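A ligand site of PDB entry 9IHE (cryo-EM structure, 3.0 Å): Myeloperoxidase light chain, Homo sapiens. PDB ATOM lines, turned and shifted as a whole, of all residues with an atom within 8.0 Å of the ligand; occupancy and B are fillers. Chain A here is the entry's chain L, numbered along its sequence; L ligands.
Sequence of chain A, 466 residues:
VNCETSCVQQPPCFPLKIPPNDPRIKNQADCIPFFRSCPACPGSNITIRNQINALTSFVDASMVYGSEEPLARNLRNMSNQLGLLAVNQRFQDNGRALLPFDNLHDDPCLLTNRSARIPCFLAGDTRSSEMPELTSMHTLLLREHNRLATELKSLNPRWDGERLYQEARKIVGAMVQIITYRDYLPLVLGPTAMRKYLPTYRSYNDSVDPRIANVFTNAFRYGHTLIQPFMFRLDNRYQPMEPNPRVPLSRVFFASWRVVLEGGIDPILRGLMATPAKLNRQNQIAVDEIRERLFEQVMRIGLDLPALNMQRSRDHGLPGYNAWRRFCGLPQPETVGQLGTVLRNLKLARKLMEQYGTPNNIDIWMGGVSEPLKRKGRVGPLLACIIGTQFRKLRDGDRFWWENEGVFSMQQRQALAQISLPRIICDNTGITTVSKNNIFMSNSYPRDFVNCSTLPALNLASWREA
N of Val 87 sits at hydrogen-bond distance from O5 of the ligand (2.5 Å). An oxygen (O5) of the ligand lies close to the backbone carbonyl oxygen of Leu 85. O3 of the ligand lies within hydrogen-bond range of OG of Ser 79 (2.8 Å). An oxygen (O4) of the ligand is in hydrogen-bond range of the side-chain amide nitrogen of Asn 80 (3.2 Å). An oxygen (O3) of the ligand sits close to the side-chain amide nitrogen of Asn 77 (3.4 Å). The side-chain amide nitrogen (NE2) of Gln 89 lies close to a nitrogen (N1) of the ligand (3.5 Å).
The backbone carbonyl oxygen (O) of Val 87 lies within hydrogen-bond range of the side-chain amide nitrogen (NE2) of Gln 89. The backbone NH (N) of Leu 85 lies within hydrogen-bond range of the side-chain amide oxygen (OD1) of Asn 146 (3.1 Å). The side-chain hydroxyl (OG) of Ser 79 sits at hydrogen-bond distance from the side-chain amide oxygen (OD1) of Asn 77. The backbone NH of Ala 86 lies within hydrogen-bond range of the backbone carbonyl oxygen of Leu 75 (3.0 Å). N of Asn 77 lies within hydrogen-bond range of O of Leu 84 (3.2 Å).
Leu 84 touches the ligand. C of Ala 86 touches O5 of the ligand, 3.1 Å away. Hydrophobic or aromatic side chains that line the ligand: Leu 84 and Val 87. Of the 21 residues printed, 8 come within 4 Å of the ligand. The nearest printed residue that does not touch the ligand is Asn 146 (4.4 Å).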
ATOM      1  N   LEU A  75     -14.823  -3.392  23.155  1.00  0.00           N
ATOM      2  CA  LEU A  75     -14.339  -4.560  22.440  1.00  0.00           C
ATOM      3  C   LEU A  75     -13.187  -4.235  21.497  1.00  0.00           C
ATOM      4  O   LEU A  75     -12.341  -5.101  21.248  1.00  0.00           O
ATOM      5  CB  LEU A  75     -15.483  -5.213  21.667  1.00  0.00           C
ATOM      6  CG  LEU A  75     -16.442  -6.054  22.507  1.00  0.00           C
ATOM      7  CD1 LEU A  75     -17.718  -6.345  21.740  1.00  0.00           C
ATOM      8  CD2 LEU A  75     -15.772  -7.349  22.948  1.00  0.00           C
ATOM      9  N   ARG A  76     -13.130  -3.019  20.971  1.00  0.00           N
ATOM     10  CA  ARG A  76     -12.117  -2.673  19.985  1.00  0.00           C
ATOM     11  C   ARG A  76     -10.764  -2.446  20.629  1.00  0.00           C
ATOM     12  O   ARG A  76     -10.621  -2.372  21.855  1.00  0.00           O
ATOM     13  CB  ARG A  76     -12.522  -1.422  19.209  1.00  0.00           C
ATOM     14  CG  ARG A  76     -13.987  -1.324  18.884  1.00  0.00           C
ATOM     15  CD  ARG A  76     -14.306   0.000  18.229  1.00  0.00           C
ATOM     16  NE  ARG A  76     -13.198   0.472  17.402  1.00  0.00           N
ATOM     17  CZ  ARG A  76     -13.257   1.522  16.611  1.00  0.00           C
ATOM     18  NH1 ARG A  76     -14.356   2.252  16.501  1.00  0.00           N
ATOM     19  NH2 ARG A  76     -12.185   1.872  15.906  1.00  0.00           N
ATOM     20  N   ASN A  77      -9.745  -2.340  19.785  1.00  0.00           N
ATOM     21  CA  ASN A  77      -8.385  -2.027  20.213  1.00  0.00           C
ATOM     22  C   ASN A  77      -8.144  -0.530  20.038  1.00  0.00           C
ATOM     23  O   ASN A  77      -8.042  -0.039  18.911  1.00  0.00           O
ATOM     24  CB  ASN A  77      -7.366  -2.838  19.416  1.00  0.00           C
ATOM     25  CG  ASN A  77      -5.977  -2.763  20.007  1.00  0.00           C
ATOM     26  OD1 ASN A  77      -5.781  -2.257  21.116  1.00  0.00           O
ATOM     27  ND2 ASN A  77      -4.986  -3.260  19.273  1.00  0.00           N
ATOM     28  N   MET A  78      -8.061   0.192  21.145  1.00  0.00           N
ATOM     29  CA  MET A  78      -7.827   1.628  21.130  1.00  0.00           C
ATOM     30  C   MET A  78      -6.359   1.987  21.331  1.00  0.00           C
ATOM     31  O   MET A  78      -6.024   3.177  21.321  1.00  0.00           O
ATOM     32  CB  MET A  78      -8.684   2.316  22.189  1.00  0.00           C
ATOM     33  CG  MET A  78     -10.176   2.192  21.951  1.00  0.00           C
ATOM     34  SD  MET A  78     -10.595   2.232  20.197  1.00  0.00           S
ATOM     35  CE  MET A  78     -11.888   3.467  20.176  1.00  0.00           C
ATOM     36  N   SER A  79      -5.486   1.005  21.527  1.00  0.00           N
ATOM     37  CA  SER A  79      -4.063   1.246  21.746  1.00  0.00           C
ATOM     38  C   SER A  79      -3.253   1.165  20.448  1.00  0.00           C
ATOM     39  O   SER A  79      -2.054   0.881  20.495  1.00  0.00           O
ATOM     40  CB  SER A  79      -3.518   0.255  22.774  1.00  0.00           C
ATOM     41  OG  SER A  79      -3.268  -1.012  22.196  1.00  0.00           O
ATOM     42  N   ASN A  80      -3.882   1.390  19.303  1.00  0.00           N
ATOM     43  CA  ASN A  80      -3.207   1.311  18.019  1.00  0.00           C
ATOM     44  C   ASN A  80      -4.028   2.062  16.991  1.00  0.00           C
ATOM     45  O   ASN A  80      -5.100   2.597  17.290  1.00  0.00           O
ATOM     46  CB  ASN A  80      -2.987  -0.151  17.601  1.00  0.00           C
ATOM     47  CG  ASN A  80      -1.606  -0.391  17.043  1.00  0.00           C
ATOM     48  OD1 ASN A  80      -1.150   0.321  16.155  1.00  0.00           O
ATOM     49  ND2 ASN A  80      -0.924  -1.400  17.565  1.00  0.00           N
ATOM     50  N   GLN A  81      -3.523   2.101  15.751  1.00  0.00           N
ATOM     51  CA  GLN A  81      -4.233   2.704  14.632  1.00  0.00           C
ATOM     52  C   GLN A  81      -4.552   1.680  13.554  1.00  0.00           C
ATOM     53  O   GLN A  81      -4.824   2.047  12.411  1.00  0.00           O
ATOM     54  CB  GLN A  81      -3.427   3.858  14.036  1.00  0.00           C
ATOM     55  CG  GLN A  81      -3.639   5.183  14.757  1.00  0.00           C
ATOM     56  CD  GLN A  81      -5.115   5.485  14.965  1.00  0.00           C
ATOM     57  OE1 GLN A  81      -5.656   5.261  16.042  1.00  0.00           O
ATOM     58  NE2 GLN A  81      -5.766   5.995  13.926  1.00  0.00           N
ATOM     59  N   LEU A  82      -4.523   0.390  13.898  1.00  0.00           N
ATOM     60  CA  LEU A  82      -4.858  -0.662  12.950  1.00  0.00           C
ATOM     61  C   LEU A  82      -6.334  -1.037  12.977  1.00  0.00           C
ATOM     62  O   LEU A  82      -6.770  -1.823  12.125  1.00  0.00           O
ATOM     63  CB  LEU A  82      -4.012  -1.911  13.230  1.00  0.00           C
ATOM     64  CG  LEU A  82      -2.593  -1.647  13.742  1.00  0.00           C
ATOM     65  CD1 LEU A  82      -1.959  -2.925  14.266  1.00  0.00           C
ATOM     66  CD2 LEU A  82      -1.733  -1.035  12.646  1.00  0.00           C
ATOM     67  N   GLY A  83      -7.111  -0.501  13.914  1.00  0.00           N
ATOM     68  CA  GLY A  83      -8.532  -0.781  13.967  1.00  0.00           C
ATOM     69  C   GLY A  83      -8.866  -2.232  14.230  1.00  0.00           C
ATOM     70  O   GLY A  83      -9.847  -2.751  13.666  1.00  0.00           O
ATOM     71  N   LEU A  84      -8.090  -2.894  15.080  1.00  0.00           N
ATOM     72  CA  LEU A  84      -8.290  -4.310  15.352  1.00  0.00           C
ATOM     73  C   LEU A  84      -9.327  -4.488  16.459  1.00  0.00           C
ATOM     74  O   LEU A  84     -10.007  -3.536  16.858  1.00  0.00           O
ATOM     75  CB  LEU A  84      -6.951  -4.956  15.731  1.00  0.00           C
ATOM     76  CG  LEU A  84      -6.221  -5.740  14.643  1.00  0.00           C
ATOM     77  CD1 LEU A  84      -6.027  -4.884  13.405  1.00  0.00           C
ATOM     78  CD2 LEU A  84      -4.890  -6.253  15.161  1.00  0.00           C
ATOM     79  N   LEU A  85      -9.465  -5.714  16.946  1.00  0.00           N
ATOM     80  CA  LEU A  85     -10.325  -6.032  18.076  1.00  0.00           C
ATOM     81  C   LEU A  85      -9.488  -6.657  19.175  1.00  0.00           C
ATOM     82  O   LEU A  85      -8.617  -7.486  18.904  1.00  0.00           O
ATOM     83  CB  LEU A  85     -11.457  -6.981  17.660  1.00  0.00           C
ATOM     84  CG  LEU A  85     -12.869  -6.403  17.645  1.00  0.00           C
ATOM     85  CD1 LEU A  85     -12.987  -5.308  16.600  1.00  0.00           C
ATOM     86  CD2 LEU A  85     -13.877  -7.499  17.381  1.00  0.00           C
ATOM     87  N   ALA A  86      -9.752  -6.251  20.423  1.00  0.00           N
ATOM     88  CA  ALA A  86      -8.927  -6.679  21.535  1.00  0.00           C
ATOM     89  C   ALA A  86      -8.981  -8.192  21.719  1.00  0.00           C
ATOM     90  O   ALA A  86     -10.041  -8.812  21.616  1.00  0.00           O
ATOM     91  CB  ALA A  86      -9.389  -5.982  22.823  1.00  0.00           C
ATOM     92  N   VAL A  87      -7.817  -8.783  21.995  1.00  0.00           N
ATOM     93  CA  VAL A  87      -7.710 -10.208  22.277  1.00  0.00           C
ATOM     94  C   VAL A  87      -7.118 -10.382  23.675  1.00  0.00           C
ATOM     95  O   VAL A  87      -6.767  -9.412  24.352  1.00  0.00           O
ATOM     96  CB  VAL A  87      -6.864 -10.960  21.231  1.00  0.00           C
ATOM     97  CG1 VAL A  87      -7.361 -10.662  19.822  1.00  0.00           C
ATOM     98  CG2 VAL A  87      -5.393 -10.621  21.382  1.00  0.00           C
ATOM     99  N   ASN A  88      -7.012 -11.638  24.098  1.00  0.00           N
ATOM    100  CA  ASN A  88      -6.445 -11.952  25.399  1.00  0.00           C
ATOM    101  C   ASN A  88      -4.964 -11.605  25.415  1.00  0.00           C
ATOM    102  O   ASN A  88      -4.231 -11.909  24.474  1.00  0.00           O
ATOM    103  CB  ASN A  88      -6.652 -13.430  25.725  1.00  0.00           C
ATOM    104  CG  ASN A  88      -7.034 -13.658  27.177  1.00  0.00           C
ATOM    105  OD1 ASN A  88      -6.185 -13.670  28.065  1.00  0.00           O
ATOM    106  ND2 ASN A  88      -8.328 -13.835  27.421  1.00  0.00           N
ATOM    107  N   GLN A  89      -4.525 -10.978  26.499  1.00  0.00           N
ATOM    108  CA  GLN A  89      -3.145 -10.529  26.632  1.00  0.00           C
ATOM    109  C   GLN A  89      -2.230 -11.537  27.313  1.00  0.00           C
ATOM    110  O   GLN A  89      -1.020 -11.327  27.352  1.00  0.00           O
ATOM    111  CB  GLN A  89      -3.096  -9.204  27.402  1.00  0.00           C
ATOM    112  CG  GLN A  89      -4.008  -8.116  26.863  1.00  0.00           C
ATOM    113  CD  GLN A  89      -3.687  -7.744  25.423  1.00  0.00           C
ATOM    114  OE1 GLN A  89      -2.555  -7.387  25.105  1.00  0.00           O
ATOM    115  NE2 GLN A  89      -4.680  -7.836  24.556  1.00  0.00           N
ATOM    116  N   GLN A  92      -2.324 -17.700  24.660  1.00  0.00           N
ATOM    117  CA  GLN A  92      -2.327 -17.836  23.220  1.00  0.00           C
ATOM    118  C   GLN A  92      -2.258 -19.315  22.854  1.00  0.00           C
ATOM    119  O   GLN A  92      -1.494 -20.067  23.454  1.00  0.00           O
ATOM    120  CB  GLN A  92      -1.149 -17.090  22.582  1.00  0.00           C
ATOM    121  CG  GLN A  92      -1.409 -15.609  22.354  1.00  0.00           C
ATOM    122  CD  GLN A  92      -0.487 -15.014  21.310  1.00  0.00           C
ATOM    123  OE1 GLN A  92       0.721 -15.268  21.313  1.00  0.00           O
ATOM    124  NE2 GLN A  92      -1.051 -14.221  20.409  1.00  0.00           N
ATOM    125  N   ALA A  97      -4.473 -15.798  18.514  1.00  0.00           N
ATOM    126  CA  ALA A  97      -5.211 -14.955  19.443  1.00  0.00           C
ATOM    127  C   ALA A  97      -6.366 -15.713  20.096  1.00  0.00           C
ATOM    128  O   ALA A  97      -6.914 -16.671  19.536  1.00  0.00           O
ATOM    129  CB  ALA A  97      -5.747 -13.714  18.718  1.00  0.00           C
ATOM    130  N   LEU A  98      -6.735 -15.261  21.294  1.00  0.00           N
ATOM    131  CA  LEU A  98      -7.862 -15.796  22.039  1.00  0.00           C
ATOM    132  C   LEU A  98      -8.759 -14.648  22.470  1.00  0.00           C
ATOM    133  O   LEU A  98      -8.383 -13.488  22.414  1.00  0.00           O
ATOM    134  CB  LEU A  98      -7.391 -16.612  23.258  1.00  0.00           C
ATOM    135  CG  LEU A  98      -7.288 -18.117  23.039  1.00  0.00           C
ATOM    136  CD1 LEU A  98      -6.085 -18.442  22.194  1.00  0.00           C
ATOM    137  CD2 LEU A  98      -7.216 -18.845  24.367  1.00  0.00           C
ATOM    138  N   PRO A 100     -10.710 -11.925  24.587  1.00  0.00           N
ATOM    139  CA  PRO A 100     -10.350 -11.174  25.794  1.00  0.00           C
ATOM    140  C   PRO A 100     -11.179 -11.612  26.996  1.00  0.00           C
ATOM    141  O   PRO A 100     -12.326 -12.036  26.860  1.00  0.00           O
ATOM    142  CB  PRO A 100     -10.651  -9.717  25.413  1.00  0.00           C
ATOM    143  CG  PRO A 100     -11.642  -9.815  24.313  1.00  0.00           C
ATOM    144  CD  PRO A 100     -11.294 -11.066  23.551  1.00  0.00           C
ATOM    145  N   LEU A 142     -13.405 -13.733  15.612  1.00  0.00           N
ATOM    146  CA  LEU A 142     -12.499 -12.652  16.009  1.00  0.00           C
ATOM    147  C   LEU A 142     -11.201 -12.696  15.216  1.00  0.00           C
ATOM    148  O   LEU A 142     -10.708 -11.671  14.735  1.00  0.00           O
ATOM    149  CB  LEU A 142     -12.221 -12.735  17.509  1.00  0.00           C
ATOM    150  CG  LEU A 142     -11.018 -11.955  18.032  1.00  0.00           C
ATOM    151  CD1 LEU A 142     -11.398 -10.515  18.309  1.00  0.00           C
ATOM    152  CD2 LEU A 142     -10.457 -12.624  19.281  1.00  0.00           C
ATOM    153  N   ASN A 146      -9.666  -9.872  12.638  1.00  0.00           N
ATOM    154  CA  ASN A 146      -8.330  -9.311  12.791  1.00  0.00           C
ATOM    155  C   ASN A 146      -7.484  -9.524  11.530  1.00  0.00           C
ATOM    156  O   ASN A 146      -6.770  -8.616  11.095  1.00  0.00           O
ATOM    157  CB  ASN A 146      -7.640  -9.929  14.001  1.00  0.00           C
ATOM    158  CG  ASN A 146      -7.914  -9.159  15.274  1.00  0.00           C
ATOM    159  OD1 ASN A 146      -8.561  -8.115  15.257  1.00  0.00           O
ATOM    160  ND2 ASN A 146      -7.412  -9.669  16.401  1.00  0.00           N
HETATM  161  C1  LIG L   1      -3.687  -4.551  21.970  1.00  0.00           C
HETATM  162  C2  LIG L   1      -3.457  -5.859  21.222  1.00  0.00           C
HETATM  163  C3  LIG L   1      -2.200  -6.500  21.811  1.00  0.00           C
HETATM  164  C4  LIG L   1      -1.032  -5.547  21.560  1.00  0.00           C
HETATM  165  C5  LIG L   1      -1.354  -4.139  22.096  1.00  0.00           C
HETATM  166  C6  LIG L   1      -0.345  -3.102  21.675  1.00  0.00           C
HETATM  167  C7  LIG L   1      -5.297  -7.106  20.204  1.00  0.00           C
HETATM  168  C8  LIG L   1      -4.786  -6.607  18.882  1.00  0.00           C
HETATM  169  N1  LIG L   1      -4.608  -6.716  21.293  1.00  0.00           N
HETATM  170  O1  LIG L   1      -2.011  -7.744  21.205  1.00  0.00           O
HETATM  171  O2  LIG L   1       0.091  -6.108  22.199  1.00  0.00           O
HETATM  172  O3  LIG L   1      -2.621  -3.693  21.644  1.00  0.00           O
HETATM  173  O4  LIG L   1      -0.353  -2.980  20.268  1.00  0.00           O
HETATM  174  O5  LIG L   1      -6.275  -7.833  20.270  1.00  0.00           O
